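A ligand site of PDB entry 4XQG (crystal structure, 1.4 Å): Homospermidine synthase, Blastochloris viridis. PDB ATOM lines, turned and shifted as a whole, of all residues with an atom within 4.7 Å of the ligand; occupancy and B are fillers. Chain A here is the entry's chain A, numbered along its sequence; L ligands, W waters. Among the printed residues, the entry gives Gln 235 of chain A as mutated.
OD1 of Asp 43 sits at hydrogen-bond distance from O6 of the ligand (2.6 Å).
An oxygen (O2) of the ligand sits at hydrogen-bond distance from the backbone NH (N) of Ser 19, at 3.0 Å.
The side-chain hydroxyl (OG) of Ser 19 lies within hydrogen-bond range of an oxygen (O9) of the ligand (2.7 Å).
An oxygen (O9) of the ligand sits at hydrogen-bond distance from the backbone NH of Ser 228.
OG of Ser 228 is in hydrogen-bond range of O1 of the ligand (2.8 Å).
N of Ile 20 is in hydrogen-bond range of O8 of the ligand (2.8 Å).
The backbone NH (N) of Ala 159 is in hydrogen-bond range of an oxygen (O14) of the ligand (2.9 Å).
The backbone NH of Val 64 is in hydrogen-bond range of a nitrogen (N4) of the ligand.
The backbone carbonyl oxygen (O) of Val 64 lies within hydrogen-bond range of a nitrogen (N3) of the ligand.
N of Asn 160 lies within hydrogen-bond range of O14 of the ligand (2.9 Å).
The backbone carbonyl oxygen of Ser 90 is in hydrogen-bond range of an oxygen (O12) of the ligand, at 2.9 Å.
O of Thr 112 sits at hydrogen-bond distance from N7 of the ligand, at 2.9 Å.
The side-chain hydroxyl of Thr 112 sits at hydrogen-bond distance from an oxygen (O11) of the ligand (3.0 Å).
The backbone carbonyl oxygen (O) of Pro 161 lies within hydrogen-bond range of a nitrogen (N7) of the ligand (3.0 Å).
The backbone carbonyl oxygen (O) of Asp 43 lies within hydrogen-bond range of the backbone NH (N) of Gln 62 (3.4 Å).
OG of Ser 90 sits at hydrogen-bond distance from OG1 of Thr 93, 2.6 Å away.
O of Ile 15 is in hydrogen-bond range of N of Ser 90.
The guanidinium group (NE) of Arg 22 sits close to the backbone carbonyl oxygen (O) of Gly 18, 3.4 Å away.
The backbone NH (N) of Leu 89 sits at hydrogen-bond distance from the backbone carbonyl oxygen (O) of Ile 15.
N of Ala 48 is in hydrogen-bond range of OG of Ser 45, at 3.1 Å.
The guanidinium group (NE) of Arg 22 lies within hydrogen-bond range of the backbone carbonyl oxygen (O) of Phe 17, 2.8 Å away.
The backbone NH (N) of Asp 92 lies within hydrogen-bond range of the side-chain carboxylate (OE2) of Glu 115 (2.9 Å).
O of Val 91 sits close to N2 of the ligand (3.3 Å).
Residues that only touch the ligand: Ile 15 (3.8 Å), Phe 17 (3.8 Å), Gly 18 (3.3 Å), Pro 44 (3.4 Å), Ser 45 (3.6 Å), Ala 63 (3.5 Å), Leu 89 (3.4 Å), Asp 92 (3.9 Å), Thr 93 (3.6 Å), Val 113 (3.5 Å), Gly 158 (3.6 Å), Trp 227 (3.5 Å), Ile 348 (3.3 Å) and Val 398 (3.5 Å).
Hydrophobic or aromatic side chains that line the ligand: Ile 15, Ile 20, Pro 44, Ala 63, Val 64, Val 91, Val 113, Ala 159, Pro 161, Trp 227, Ile 348 and Val 398.
25 residues have an atom within 4 Å of the ligand: Ile 15, Phe 17, Gly 18, Ser 19, Ile 20, Asp 43, Pro 44, Ser 45, Ala 63, Val 64, Leu 89, Ser 90, Val 91, Asp 92, Thr 93, Thr 112, Val 113, Gly 158, Ala 159, Asn 160, Pro 161, Trp 227, Ser 228, Ile 348 and Val 398.
Water W3 bridges an oxygen (O5) of the ligand (2.5 Å) and the guanidinium group of Arg 22 (3.0 Å).
Water W4 lies within hydrogen-bond range of O8 of the ligand (2.7 Å), O of Leu 89 (2.8 Å), N of Gly 18 (2.9 Å) and N of Gly 21 (2.9 Å).
Water W6 bridges the side-chain carboxylate of Asp 92 (2.7 Å) and a nitrogen (N2) of the ligand (2.8 Å).
Water W12 bridges O13 of the ligand and OE1 of Gln 235.
Water W1 lies within hydrogen-bond range of the backbone carbonyl oxygen (O) of Asn 160 (2.9 Å) and an oxygen (O14) of the ligand (3.5 Å).
Water W11 lies within hydrogen-bond range of O of Asp 92 (2.8 Å), O of Val 64 (2.8 Å) and N3 of the ligand (3.4 Å).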
ATOM      1  N   ILE A  15       6.626  -7.653 -11.127  1.00  0.00           N
ATOM      2  CA  ILE A  15       7.316  -7.218  -9.914  1.00  0.00           C
ATOM      3  C   ILE A  15       6.871  -5.788  -9.664  1.00  0.00           C
ATOM      4  O   ILE A  15       7.196  -4.870 -10.439  1.00  0.00           O
ATOM      5  CB  ILE A  15       8.850  -7.282 -10.061  1.00  0.00           C
ATOM      6  CG1 ILE A  15       9.304  -8.671 -10.493  1.00  0.00           C
ATOM      7  CG2 ILE A  15       9.519  -6.927  -8.744  1.00  0.00           C
ATOM      8  CD1 ILE A  15      10.823  -8.790 -10.751  1.00  0.00           C
ATOM      9  N   GLY A  16       6.143  -5.593  -8.570  1.00  0.00           N
ATOM     10  CA  GLY A  16       5.611  -4.296  -8.212  1.00  0.00           C
ATOM     11  C   GLY A  16       4.149  -4.134  -8.602  1.00  0.00           C
ATOM     12  O   GLY A  16       3.760  -4.402  -9.736  1.00  0.00           O
ATOM     13  N   PHE A  17       3.347  -3.668  -7.657  1.00  0.00           N
ATOM     14  CA  PHE A  17       1.919  -3.460  -7.890  1.00  0.00           C
ATOM     15  C   PHE A  17       1.503  -2.151  -7.232  1.00  0.00           C
ATOM     16  O   PHE A  17       0.566  -2.107  -6.430  1.00  0.00           O
ATOM     17  CB  PHE A  17       1.126  -4.654  -7.361  1.00  0.00           C
ATOM     18  CG  PHE A  17      -0.266  -4.779  -7.944  1.00  0.00           C
ATOM     19  CD1 PHE A  17      -0.453  -4.920  -9.321  1.00  0.00           C
ATOM     20  CD2 PHE A  17      -1.380  -4.795  -7.124  1.00  0.00           C
ATOM     21  CE1 PHE A  17      -1.706  -5.067  -9.844  1.00  0.00           C
ATOM     22  CE2 PHE A  17      -2.649  -4.934  -7.662  1.00  0.00           C
ATOM     23  CZ  PHE A  17      -2.805  -5.057  -9.020  1.00  0.00           C
ATOM     24  N   GLY A  18       2.218  -1.089  -7.586  1.00  0.00           N
ATOM     25  CA  GLY A  18       1.850   0.261  -7.229  1.00  0.00           C
ATOM     26  C   GLY A  18       1.043   0.886  -8.361  1.00  0.00           C
ATOM     27  O   GLY A  18       0.301   0.178  -9.042  1.00  0.00           O
ATOM     28  N   SER A  19       1.175   2.186  -8.564  1.00  0.00           N
ATOM     29  CA  SER A  19       0.266   2.845  -9.509  1.00  0.00           C
ATOM     30  C   SER A  19       0.423   2.254 -10.917  1.00  0.00           C
ATOM     31  O   SER A  19      -0.565   2.067 -11.629  1.00  0.00           O
ATOM     32  CB  SER A  19       0.425   4.362  -9.470  1.00  0.00           C
ATOM     33  OG  SER A  19       1.452   4.835 -10.310  1.00  0.00           O
ATOM     34  N   ILE A  20       1.652   1.957 -11.321  1.00  0.00           N
ATOM     35  CA  ILE A  20       1.863   1.463 -12.677  1.00  0.00           C
ATOM     36  C   ILE A  20       1.470  -0.014 -12.835  1.00  0.00           C
ATOM     37  O   ILE A  20       0.795  -0.384 -13.801  1.00  0.00           O
ATOM     38  CB  ILE A  20       3.289   1.736 -13.165  1.00  0.00           C
ATOM     39  CG1 ILE A  20       3.610   3.248 -13.083  1.00  0.00           C
ATOM     40  CG2 ILE A  20       3.489   1.182 -14.590  1.00  0.00           C
ATOM     41  CD1 ILE A  20       2.561   4.164 -13.748  1.00  0.00           C
ATOM     42  N   GLY A  21       1.848  -0.856 -11.882  1.00  0.00           N
ATOM     43  CA  GLY A  21       1.434  -2.251 -11.932  1.00  0.00           C
ATOM     44  C   GLY A  21      -0.067  -2.374 -11.952  1.00  0.00           C
ATOM     45  O   GLY A  21      -0.613  -3.204 -12.667  1.00  0.00           O
ATOM     46  N   ARG A  22      -0.750  -1.553 -11.157  1.00  0.00           N
ATOM     47  CA  ARG A  22      -2.210  -1.586 -11.108  1.00  0.00           C
ATOM     48  C   ARG A  22      -2.844  -1.213 -12.452  1.00  0.00           C
ATOM     49  O   ARG A  22      -3.884  -1.784 -12.828  1.00  0.00           O
ATOM     50  CB  ARG A  22      -2.717  -0.663  -9.995  1.00  0.00           C
ATOM     51  CG  ARG A  22      -2.419  -1.197  -8.618  1.00  0.00           C
ATOM     52  CD  ARG A  22      -2.601  -0.163  -7.521  1.00  0.00           C
ATOM     53  NE  ARG A  22      -1.750  -0.548  -6.391  1.00  0.00           N
ATOM     54  CZ  ARG A  22      -1.756   0.009  -5.191  1.00  0.00           C
ATOM     55  NH1 ARG A  22      -2.580   1.028  -4.916  1.00  0.00           N
ATOM     56  NH2 ARG A  22      -0.921  -0.450  -4.270  1.00  0.00           N
ATOM     57  N   ILE A  42       4.336  -9.772  -7.471  1.00  0.00           N
ATOM     58  CA  ILE A  42       5.189  -9.772  -6.301  1.00  0.00           C
ATOM     59  C   ILE A  42       5.343  -8.341  -5.788  1.00  0.00           C
ATOM     60  O   ILE A  42       5.807  -7.466  -6.494  1.00  0.00           O
ATOM     61  CB  ILE A  42       6.607 -10.316  -6.643  1.00  0.00           C
ATOM     62  CG1 ILE A  42       6.539 -11.662  -7.363  1.00  0.00           C
ATOM     63  CG2 ILE A  42       7.470 -10.376  -5.379  1.00  0.00           C
ATOM     64  CD1 ILE A  42       7.893 -12.151  -7.877  1.00  0.00           C
ATOM     65  N   ASP A  43       4.950  -8.096  -4.539  1.00  0.00           N
ATOM     66  CA  ASP A  43       5.081  -6.755  -3.962  1.00  0.00           C
ATOM     67  C   ASP A  43       4.953  -6.897  -2.440  1.00  0.00           C
ATOM     68  O   ASP A  43       4.121  -7.655  -1.974  1.00  0.00           O
ATOM     69  CB  ASP A  43       3.959  -5.865  -4.522  1.00  0.00           C
ATOM     70  CG  ASP A  43       4.115  -4.396  -4.151  1.00  0.00           C
ATOM     71  OD1 ASP A  43       4.215  -4.051  -2.954  1.00  0.00           O
ATOM     72  OD2 ASP A  43       4.094  -3.559  -5.072  1.00  0.00           O
ATOM     73  N   PRO A  44       5.815  -6.203  -1.668  1.00  0.00           N
ATOM     74  CA  PRO A  44       5.764  -6.365  -0.190  1.00  0.00           C
ATOM     75  C   PRO A  44       4.609  -5.644   0.513  1.00  0.00           C
ATOM     76  O   PRO A  44       4.393  -5.890   1.684  1.00  0.00           O
ATOM     77  CB  PRO A  44       7.079  -5.743   0.267  1.00  0.00           C
ATOM     78  CG  PRO A  44       7.422  -4.732  -0.815  1.00  0.00           C
ATOM     79  CD  PRO A  44       6.949  -5.383  -2.103  1.00  0.00           C
ATOM     80  N   SER A  45       3.890  -4.776  -0.194  1.00  0.00           N
ATOM     81  CA  SER A  45       2.888  -3.908   0.432  1.00  0.00           C
ATOM     82  C   SER A  45       1.576  -4.626   0.736  1.00  0.00           C
ATOM     83  O   SER A  45       1.044  -5.378  -0.089  1.00  0.00           O
ATOM     84  CB  SER A  45       2.616  -2.719  -0.500  1.00  0.00           C
ATOM     85  OG  SER A  45       1.367  -2.115  -0.242  1.00  0.00           O
ATOM     86  N   ALA A  48      -1.150  -3.283  -1.588  1.00  0.00           N
ATOM     87  CA  ALA A  48      -1.062  -3.954  -2.870  1.00  0.00           C
ATOM     88  C   ALA A  48      -1.702  -5.338  -2.820  1.00  0.00           C
ATOM     89  O   ALA A  48      -2.425  -5.739  -3.735  1.00  0.00           O
ATOM     90  CB  ALA A  48       0.392  -4.057  -3.311  1.00  0.00           C
ATOM     91  N   GLN A  62       6.266 -10.138  -0.925  1.00  0.00           N
ATOM     92  CA  GLN A  62       7.684 -10.255  -0.631  1.00  0.00           C
ATOM     93  C   GLN A  62       8.426  -9.128  -1.334  1.00  0.00           C
ATOM     94  O   GLN A  62       8.127  -8.807  -2.476  1.00  0.00           O
ATOM     95  CB  GLN A  62       8.207 -11.602  -1.125  1.00  0.00           C
ATOM     96  CG  GLN A  62       9.669 -11.837  -0.841  1.00  0.00           C
ATOM     97  CD  GLN A  62      10.015 -11.768   0.614  1.00  0.00           C
ATOM     98  OE1 GLN A  62      10.978 -11.117   1.006  1.00  0.00           O
ATOM     99  NE2 GLN A  62       9.210 -12.421   1.433  1.00  0.00           N
ATOM    100  N   ALA A  63       9.406  -8.556  -0.648  1.00  0.00           N
ATOM    101  CA  ALA A  63      10.327  -7.617  -1.277  1.00  0.00           C
ATOM    102  C   ALA A  63      11.432  -8.386  -1.980  1.00  0.00           C
ATOM    103  O   ALA A  63      12.027  -9.280  -1.406  1.00  0.00           O
ATOM    104  CB  ALA A  63      10.928  -6.702  -0.230  1.00  0.00           C
ATOM    105  N   VAL A  64      11.675  -8.047  -3.238  1.00  0.00           N
ATOM    106  CA  VAL A  64      12.747  -8.660  -4.006  1.00  0.00           C
ATOM    107  C   VAL A  64      14.004  -7.917  -3.619  1.00  0.00           C
ATOM    108  O   VAL A  64      14.016  -6.695  -3.626  1.00  0.00           O
ATOM    109  CB  VAL A  64      12.492  -8.547  -5.517  1.00  0.00           C
ATOM    110  CG1 VAL A  64      13.676  -9.094  -6.314  1.00  0.00           C
ATOM    111  CG2 VAL A  64      11.202  -9.237  -5.894  1.00  0.00           C
ATOM    112  N   LEU A  89       7.984  -3.415 -12.553  1.00  0.00           N
ATOM    113  CA  LEU A  89       7.326  -2.130 -12.330  1.00  0.00           C
ATOM    114  C   LEU A  89       7.494  -1.725 -10.866  1.00  0.00           C
ATOM    115  O   LEU A  89       6.572  -1.277 -10.215  1.00  0.00           O
ATOM    116  CB  LEU A  89       5.847  -2.225 -12.694  1.00  0.00           C
ATOM    117  CG  LEU A  89       5.598  -2.690 -14.136  1.00  0.00           C
ATOM    118  CD1 LEU A  89       4.105  -2.903 -14.401  1.00  0.00           C
ATOM    119  CD2 LEU A  89       6.152  -1.726 -15.179  1.00  0.00           C
ATOM    120  N   SER A  90       8.710  -1.887 -10.366  1.00  0.00           N
ATOM    121  CA  SER A  90       8.976  -1.755  -8.945  1.00  0.00           C
ATOM    122  C   SER A  90       9.882  -0.576  -8.621  1.00  0.00           C
ATOM    123  O   SER A  90      10.397   0.092  -9.505  1.00  0.00           O
ATOM    124  CB  SER A  90       9.612  -3.058  -8.430  1.00  0.00           C
ATOM    125  OG  SER A  90      10.873  -3.287  -9.053  1.00  0.00           O
ATOM    126  N   VAL A  91      10.008  -0.309  -7.326  1.00  0.00           N
ATOM    127  CA  VAL A  91      11.095   0.519  -6.824  1.00  0.00           C
ATOM    128  C   VAL A  91      12.012  -0.373  -5.982  1.00  0.00           C
ATOM    129  O   VAL A  91      11.628  -1.473  -5.583  1.00  0.00           O
ATOM    130  CB  VAL A  91      10.595   1.720  -5.967  1.00  0.00           C
ATOM    131  CG1 VAL A  91       9.689   2.641  -6.788  1.00  0.00           C
ATOM    132  CG2 VAL A  91       9.871   1.248  -4.732  1.00  0.00           C
ATOM    133  N   ASP A  92      13.219   0.117  -5.733  1.00  0.00           N
ATOM    134  CA  ASP A  92      14.154  -0.477  -4.752  1.00  0.00           C
ATOM    135  C   ASP A  92      14.785  -1.805  -5.203  1.00  0.00           C
ATOM    136  O   ASP A  92      15.427  -2.482  -4.407  1.00  0.00           O
ATOM    137  CB  ASP A  92      13.467  -0.662  -3.380  1.00  0.00           C
ATOM    138  CG  ASP A  92      13.058   0.670  -2.724  1.00  0.00           C
ATOM    139  OD1 ASP A  92      13.431   1.761  -3.200  1.00  0.00           O
ATOM    140  OD2 ASP A  92      12.366   0.603  -1.690  1.00  0.00           O
ATOM    141  N   THR A  93      14.645  -2.159  -6.475  1.00  0.00           N
ATOM    142  CA  THR A  93      15.197  -3.384  -7.025  1.00  0.00           C
ATOM    143  C   THR A  93      16.153  -3.041  -8.175  1.00  0.00           C
ATOM    144  O   THR A  93      15.986  -2.021  -8.852  1.00  0.00           O
ATOM    145  CB  THR A  93      14.093  -4.246  -7.601  1.00  0.00           C
ATOM    146  OG1 THR A  93      13.446  -3.492  -8.640  1.00  0.00           O
ATOM    147  CG2 THR A  93      13.076  -4.628  -6.537  1.00  0.00           C
ATOM    148  N   THR A 112      10.681   0.208 -16.691  1.00  0.00           N
ATOM    149  CA  THR A 112      10.404   1.597 -17.047  1.00  0.00           C
ATOM    150  C   THR A 112      11.441   2.569 -16.464  1.00  0.00           C
ATOM    151  O   THR A 112      11.227   3.770 -16.496  1.00  0.00           O
ATOM    152  CB  THR A 112       9.017   2.027 -16.564  1.00  0.00           C
ATOM    153  OG1 THR A 112       8.978   2.088 -15.137  1.00  0.00           O
ATOM    154  CG2 THR A 112       7.918   1.090 -17.080  1.00  0.00           C
ATOM    155  N   VAL A 113      12.553   2.026 -15.972  1.00  0.00           N
ATOM    156  CA  VAL A 113      13.539   2.805 -15.218  1.00  0.00           C
ATOM    157  C   VAL A 113      14.740   1.884 -14.990  1.00  0.00           C
ATOM    158  O   VAL A 113      14.567   0.668 -14.871  1.00  0.00           O
ATOM    159  CB  VAL A 113      12.968   3.255 -13.839  1.00  0.00           C
ATOM    160  CG1 VAL A 113      12.519   2.060 -12.974  1.00  0.00           C
ATOM    161  CG2 VAL A 113      13.970   4.121 -13.078  1.00  0.00           C
ATOM    162  N   GLU A 115      16.624   1.120 -12.235  1.00  0.00           N
ATOM    163  CA  GLU A 115      16.560   1.237 -10.792  1.00  0.00           C
ATOM    164  C   GLU A 115      17.714   0.456 -10.162  1.00  0.00           C
ATOM    165  O   GLU A 115      18.093  -0.590 -10.683  1.00  0.00           O
ATOM    166  CB  GLU A 115      15.207   0.695 -10.292  1.00  0.00           C
ATOM    167  CG  GLU A 115      14.902   0.868  -8.799  1.00  0.00           C
ATOM    168  CD  GLU A 115      14.494   2.280  -8.381  1.00  0.00           C
ATOM    169  OE1 GLU A 115      14.566   3.215  -9.215  1.00  0.00           O
ATOM    170  OE2 GLU A 115      14.086   2.448  -7.205  1.00  0.00           O
ATOM    171  N   GLY A 158       8.481   3.014 -20.390  1.00  0.00           N
ATOM    172  CA  GLY A 158       7.251   3.588 -19.893  1.00  0.00           C
ATOM    173  C   GLY A 158       6.827   4.742 -20.784  1.00  0.00           C
ATOM    174  O   GLY A 158       7.019   4.686 -21.993  1.00  0.00           O
ATOM    175  N   ALA A 159       6.209   5.771 -20.213  1.00  0.00           N
ATOM    176  CA  ALA A 159       5.813   6.947 -20.991  1.00  0.00           C
ATOM    177  C   ALA A 159       7.034   7.820 -21.298  1.00  0.00           C
ATOM    178  O   ALA A 159       7.199   8.292 -22.423  1.00  0.00           O
ATOM    179  CB  ALA A 159       4.756   7.749 -20.215  1.00  0.00           C
ATOM    180  N   ASN A 160       7.839   8.054 -20.272  1.00  0.00           N
ATOM    181  CA  ASN A 160       9.007   8.900 -20.387  1.00  0.00           C
ATOM    182  C   ASN A 160       9.935   8.588 -19.203  1.00  0.00           C
ATOM    183  O   ASN A 160       9.683   9.024 -18.099  1.00  0.00           O
ATOM    184  CB  ASN A 160       8.648  10.395 -20.441  1.00  0.00           C
ATOM    185  CG  ASN A 160       7.802  10.895 -19.266  1.00  0.00           C
ATOM    186  OD1 ASN A 160       6.854  10.259 -18.837  1.00  0.00           O
ATOM    187  ND2 ASN A 160       8.127  12.087 -18.784  1.00  0.00           N
ATOM    188  N   PRO A 161      10.982   7.786 -19.432  1.00  0.00           N
ATOM    189  CA  PRO A 161      11.435   7.235 -20.730  1.00  0.00           C
ATOM    190  C   PRO A 161      10.468   6.201 -21.299  1.00  0.00           C
ATOM    191  O   PRO A 161       9.774   5.525 -20.541  1.00  0.00           O
ATOM    192  CB  PRO A 161      12.757   6.556 -20.356  1.00  0.00           C
ATOM    193  CG  PRO A 161      12.586   6.203 -18.878  1.00  0.00           C
ATOM    194  CD  PRO A 161      11.849   7.365 -18.317  1.00  0.00           C
ATOM    195  N   TRP A 227       1.770   9.734  -9.611  1.00  0.00           N
ATOM    196  CA  TRP A 227       2.484   8.472  -9.782  1.00  0.00           C
ATOM    197  C   TRP A 227       3.473   8.414  -8.623  1.00  0.00           C
ATOM    198  O   TRP A 227       3.464   9.309  -7.772  1.00  0.00           O
ATOM    199  CB  TRP A 227       3.182   8.400 -11.159  1.00  0.00           C
ATOM    200  CG  TRP A 227       4.214   9.490 -11.375  1.00  0.00           C
ATOM    201  CD1 TRP A 227       3.983  10.790 -11.710  1.00  0.00           C
ATOM    202  CD2 TRP A 227       5.642   9.332 -11.304  1.00  0.00           C
ATOM    203  NE1 TRP A 227       5.192  11.462 -11.821  1.00  0.00           N
ATOM    204  CE2 TRP A 227       6.217  10.591 -11.580  1.00  0.00           C
ATOM    205  CE3 TRP A 227       6.489   8.249 -11.022  1.00  0.00           C
ATOM    206  CZ2 TRP A 227       7.591  10.785 -11.609  1.00  0.00           C
ATOM    207  CZ3 TRP A 227       7.856   8.450 -11.046  1.00  0.00           C
ATOM    208  CH2 TRP A 227       8.388   9.713 -11.324  1.00  0.00           C
ATOM    209  N   SER A 228       4.294   7.357  -8.555  1.00  0.00           N
ATOM    210  CA  SER A 228       5.224   7.125  -7.455  1.00  0.00           C
ATOM    211  C   SER A 228       5.719   8.395  -6.776  1.00  0.00           C
ATOM    212  O   SER A 228       6.385   9.232  -7.392  1.00  0.00           O
ATOM    213  CB  SER A 228       6.451   6.361  -7.939  1.00  0.00           C
ATOM    214  OG  SER A 228       7.143   5.825  -6.816  1.00  0.00           O
ATOM    215  N   VAL A 229       5.385   8.557  -5.493  1.00  0.00           N
ATOM    216  CA  VAL A 229       6.027   9.592  -4.713  1.00  0.00           C
ATOM    217  C   VAL A 229       7.477   9.198  -4.436  1.00  0.00           C
ATOM    218  O   VAL A 229       8.402  10.001  -4.593  1.00  0.00           O
ATOM    219  CB  VAL A 229       5.257   9.913  -3.416  1.00  0.00           C
ATOM    220  CG1 VAL A 229       6.095  10.846  -2.525  1.00  0.00           C
ATOM    221  CG2 VAL A 229       3.925  10.542  -3.771  1.00  0.00           C
ATOM    222  N   GLY A 231       9.448   7.213  -6.063  1.00  0.00           N
ATOM    223  CA  GLY A 231      10.230   7.289  -7.274  1.00  0.00           C
ATOM    224  C   GLY A 231      10.472   8.710  -7.757  1.00  0.00           C
ATOM    225  O   GLY A 231      11.574   9.033  -8.195  1.00  0.00           O
ATOM    226  N   GLN A 235      14.258  10.446  -7.968  1.00  0.00           N
ATOM    227  CA  GLN A 235      14.863  11.031  -9.156  1.00  0.00           C
ATOM    228  C   GLN A 235      15.042  12.537  -9.012  1.00  0.00           C
ATOM    229  O   GLN A 235      15.981  13.101  -9.537  1.00  0.00           O
ATOM    230  CB  GLN A 235      14.114  10.647 -10.451  1.00  0.00           C
ATOM    231  CG  GLN A 235      12.713  11.164 -10.575  1.00  0.00           C
ATOM    232  CD  GLN A 235      11.994  10.647 -11.826  1.00  0.00           C
ATOM    233  OE1 GLN A 235      12.117   9.459 -12.193  1.00  0.00           O
ATOM    234  NE2 GLN A 235      11.202  11.511 -12.467  1.00  0.00           N
ATOM    235  N   ILE A 348      -0.670   9.034  -3.607  1.00  0.00           N
ATOM    236  CA  ILE A 348      -0.794   9.071  -5.056  1.00  0.00           C
ATOM    237  C   ILE A 348      -2.276   9.234  -5.378  1.00  0.00           C
ATOM    238  O   ILE A 348      -3.133   8.473  -4.898  1.00  0.00           O
ATOM    239  CB  ILE A 348      -0.212   7.805  -5.696  1.00  0.00           C
ATOM    240  CG1 ILE A 348       1.277   7.695  -5.374  1.00  0.00           C
ATOM    241  CG2 ILE A 348      -0.438   7.826  -7.181  1.00  0.00           C
ATOM    242  CD1 ILE A 348       1.889   6.357  -5.815  1.00  0.00           C
ATOM    243  N   VAL A 398       1.815   5.400 -19.163  1.00  0.00           N
ATOM    244  CA  VAL A 398       2.917   4.510 -18.843  1.00  0.00           C
ATOM    245  C   VAL A 398       2.533   3.054 -19.097  1.00  0.00           C
ATOM    246  O   VAL A 398       3.287   2.302 -19.739  1.00  0.00           O
ATOM    247  CB  VAL A 398       3.319   4.663 -17.364  1.00  0.00           C
ATOM    248  CG1 VAL A 398       4.455   3.738 -17.003  1.00  0.00           C
ATOM    249  CG2 VAL A 398       3.619   6.124 -17.023  1.00  0.00           C
HETATM  250  P1  LIG L   1       4.611   3.184  -6.625  1.00  0.00           P
HETATM  251  O1  LIG L   1       5.461   3.911  -5.594  1.00  0.00           O
HETATM  252  O2  LIG L   1       3.163   3.455  -6.741  1.00  0.00           O
HETATM  253  O3  LIG L   1       4.777   1.605  -6.433  1.00  0.00           O
HETATM  254  C1  LIG L   1       6.036   0.990  -6.221  1.00  0.00           C
HETATM  255  C2  LIG L   1       5.768  -0.352  -5.760  1.00  0.00           C
HETATM  256  O4  LIG L   1       7.060  -1.092  -5.589  1.00  0.00           O
HETATM  257  C3  LIG L   1       5.122  -0.589  -4.362  1.00  0.00           C
HETATM  258  O5  LIG L   1       3.722  -1.001  -4.392  1.00  0.00           O
HETATM  259  C4  LIG L   1       5.954  -0.923  -3.479  1.00  0.00           C
HETATM  260  O6  LIG L   1       5.503  -1.811  -2.396  1.00  0.00           O
HETATM  261  C5  LIG L   1       7.025  -1.668  -4.433  1.00  0.00           C
HETATM  262  N1  LIG L   1       8.164  -2.291  -3.966  1.00  0.00           N
HETATM  263  C6  LIG L   1       8.976  -1.686  -3.099  1.00  0.00           C
HETATM  264  N2  LIG L   1      10.015  -2.409  -2.832  1.00  0.00           N
HETATM  265  C7  LIG L   1       9.910  -3.553  -3.572  1.00  0.00           C
HETATM  266  C8  LIG L   1      10.728  -4.718  -3.713  1.00  0.00           C
HETATM  267  N3  LIG L   1      11.937  -4.812  -3.005  1.00  0.00           N
HETATM  268  N4  LIG L   1      10.309  -5.690  -4.515  1.00  0.00           N
HETATM  269  C9  LIG L   1       9.165  -5.582  -5.192  1.00  0.00           C
HETATM  270  N5  LIG L   1       8.391  -4.513  -5.100  1.00  0.00           N
HETATM  271  C10 LIG L   1       8.737  -3.476  -4.295  1.00  0.00           C
HETATM  272  O7  LIG L   1       5.382   3.485  -8.003  1.00  0.00           O
HETATM  273  P2  LIG L   1       4.755   3.444  -9.505  1.00  0.00           P
HETATM  274  O8  LIG L   1       3.989   2.190  -9.731  1.00  0.00           O
HETATM  275  O9  LIG L   1       4.050   4.777  -9.776  1.00  0.00           O
HETATM  276  O10 LIG L   1       6.110   3.423 -10.353  1.00  0.00           O
HETATM  277  C11 LIG L   1       6.783   2.154 -10.399  1.00  0.00           C
HETATM  278  C12 LIG L   1       8.120   2.295 -11.116  1.00  0.00           C
HETATM  279  O11 LIG L   1       7.942   2.714 -12.356  1.00  0.00           O
HETATM  280  C13 LIG L   1       9.048   3.308 -10.419  1.00  0.00           C
HETATM  281  O12 LIG L   1      10.334   2.860 -10.371  1.00  0.00           O
HETATM  282  C14 LIG L   1       9.108   4.388 -11.443  1.00  0.00           C
HETATM  283  O13 LIG L   1      10.112   5.384 -11.235  1.00  0.00           O
HETATM  284  C15 LIG L   1       8.771   4.015 -12.648  1.00  0.00           C
HETATM  285  N6  LIG L   1       7.965   4.821 -13.495  1.00  0.00           N
HETATM  286  C16 LIG L   1       8.380   5.043 -14.761  1.00  0.00           C
HETATM  287  C17 LIG L   1       7.665   5.857 -15.601  1.00  0.00           C
HETATM  288  C18 LIG L   1       8.033   6.129 -17.054  1.00  0.00           C
HETATM  289  O14 LIG L   1       7.280   6.767 -17.760  1.00  0.00           O
HETATM  290  N7  LIG L   1       9.188   5.531 -17.582  1.00  0.00           N
HETATM  291  C19 LIG L   1       6.511   6.424 -15.122  1.00  0.00           C
HETATM  292  C20 LIG L   1       6.080   6.137 -13.824  1.00  0.00           C
HETATM  293  C21 LIG L   1       6.835   5.312 -13.053  1.00  0.00           C
HETATM  294  O   HOH W   1       8.425   9.156 -15.534  1.00  0.00           O
HETATM  295  O   HOH W   2       9.368   0.995  -1.192  1.00  0.00           O
HETATM  296  O   HOH W   3       1.839   0.475  -3.522  1.00  0.00           O
HETATM  297  O   HOH W   4       3.935  -0.507  -9.846  1.00  0.00           O
HETATM  298  O   HOH W   5      13.544  -3.872  -0.503  1.00  0.00           O
HETATM  299  O   HOH W   6      11.768  -1.814  -0.685  1.00  0.00           O
HETATM  300  O   HOH W   7       5.814  -0.729   0.022  1.00  0.00           O
HETATM  301  O   HOH W   8       5.687   9.726 -14.782  1.00  0.00           O
HETATM  302  O   HOH W   9       5.310   6.076  -3.931  1.00  0.00           O
HETATM  303  O   HOH W  10       1.149   2.874  -4.946  1.00  0.00           O
HETATM  304  O   HOH W  11      15.294  -4.466  -2.501  1.00  0.00           O
HETATM  305  O   HOH W  12      10.341   7.217 -13.653  1.00  0.00           O
HETATM  306  O   HOH W  13      12.380   4.955  -9.504  1.00  0.00           O
HETATM  307  O   HOH W  14       6.349   2.663  -3.240  1.00  0.00           O
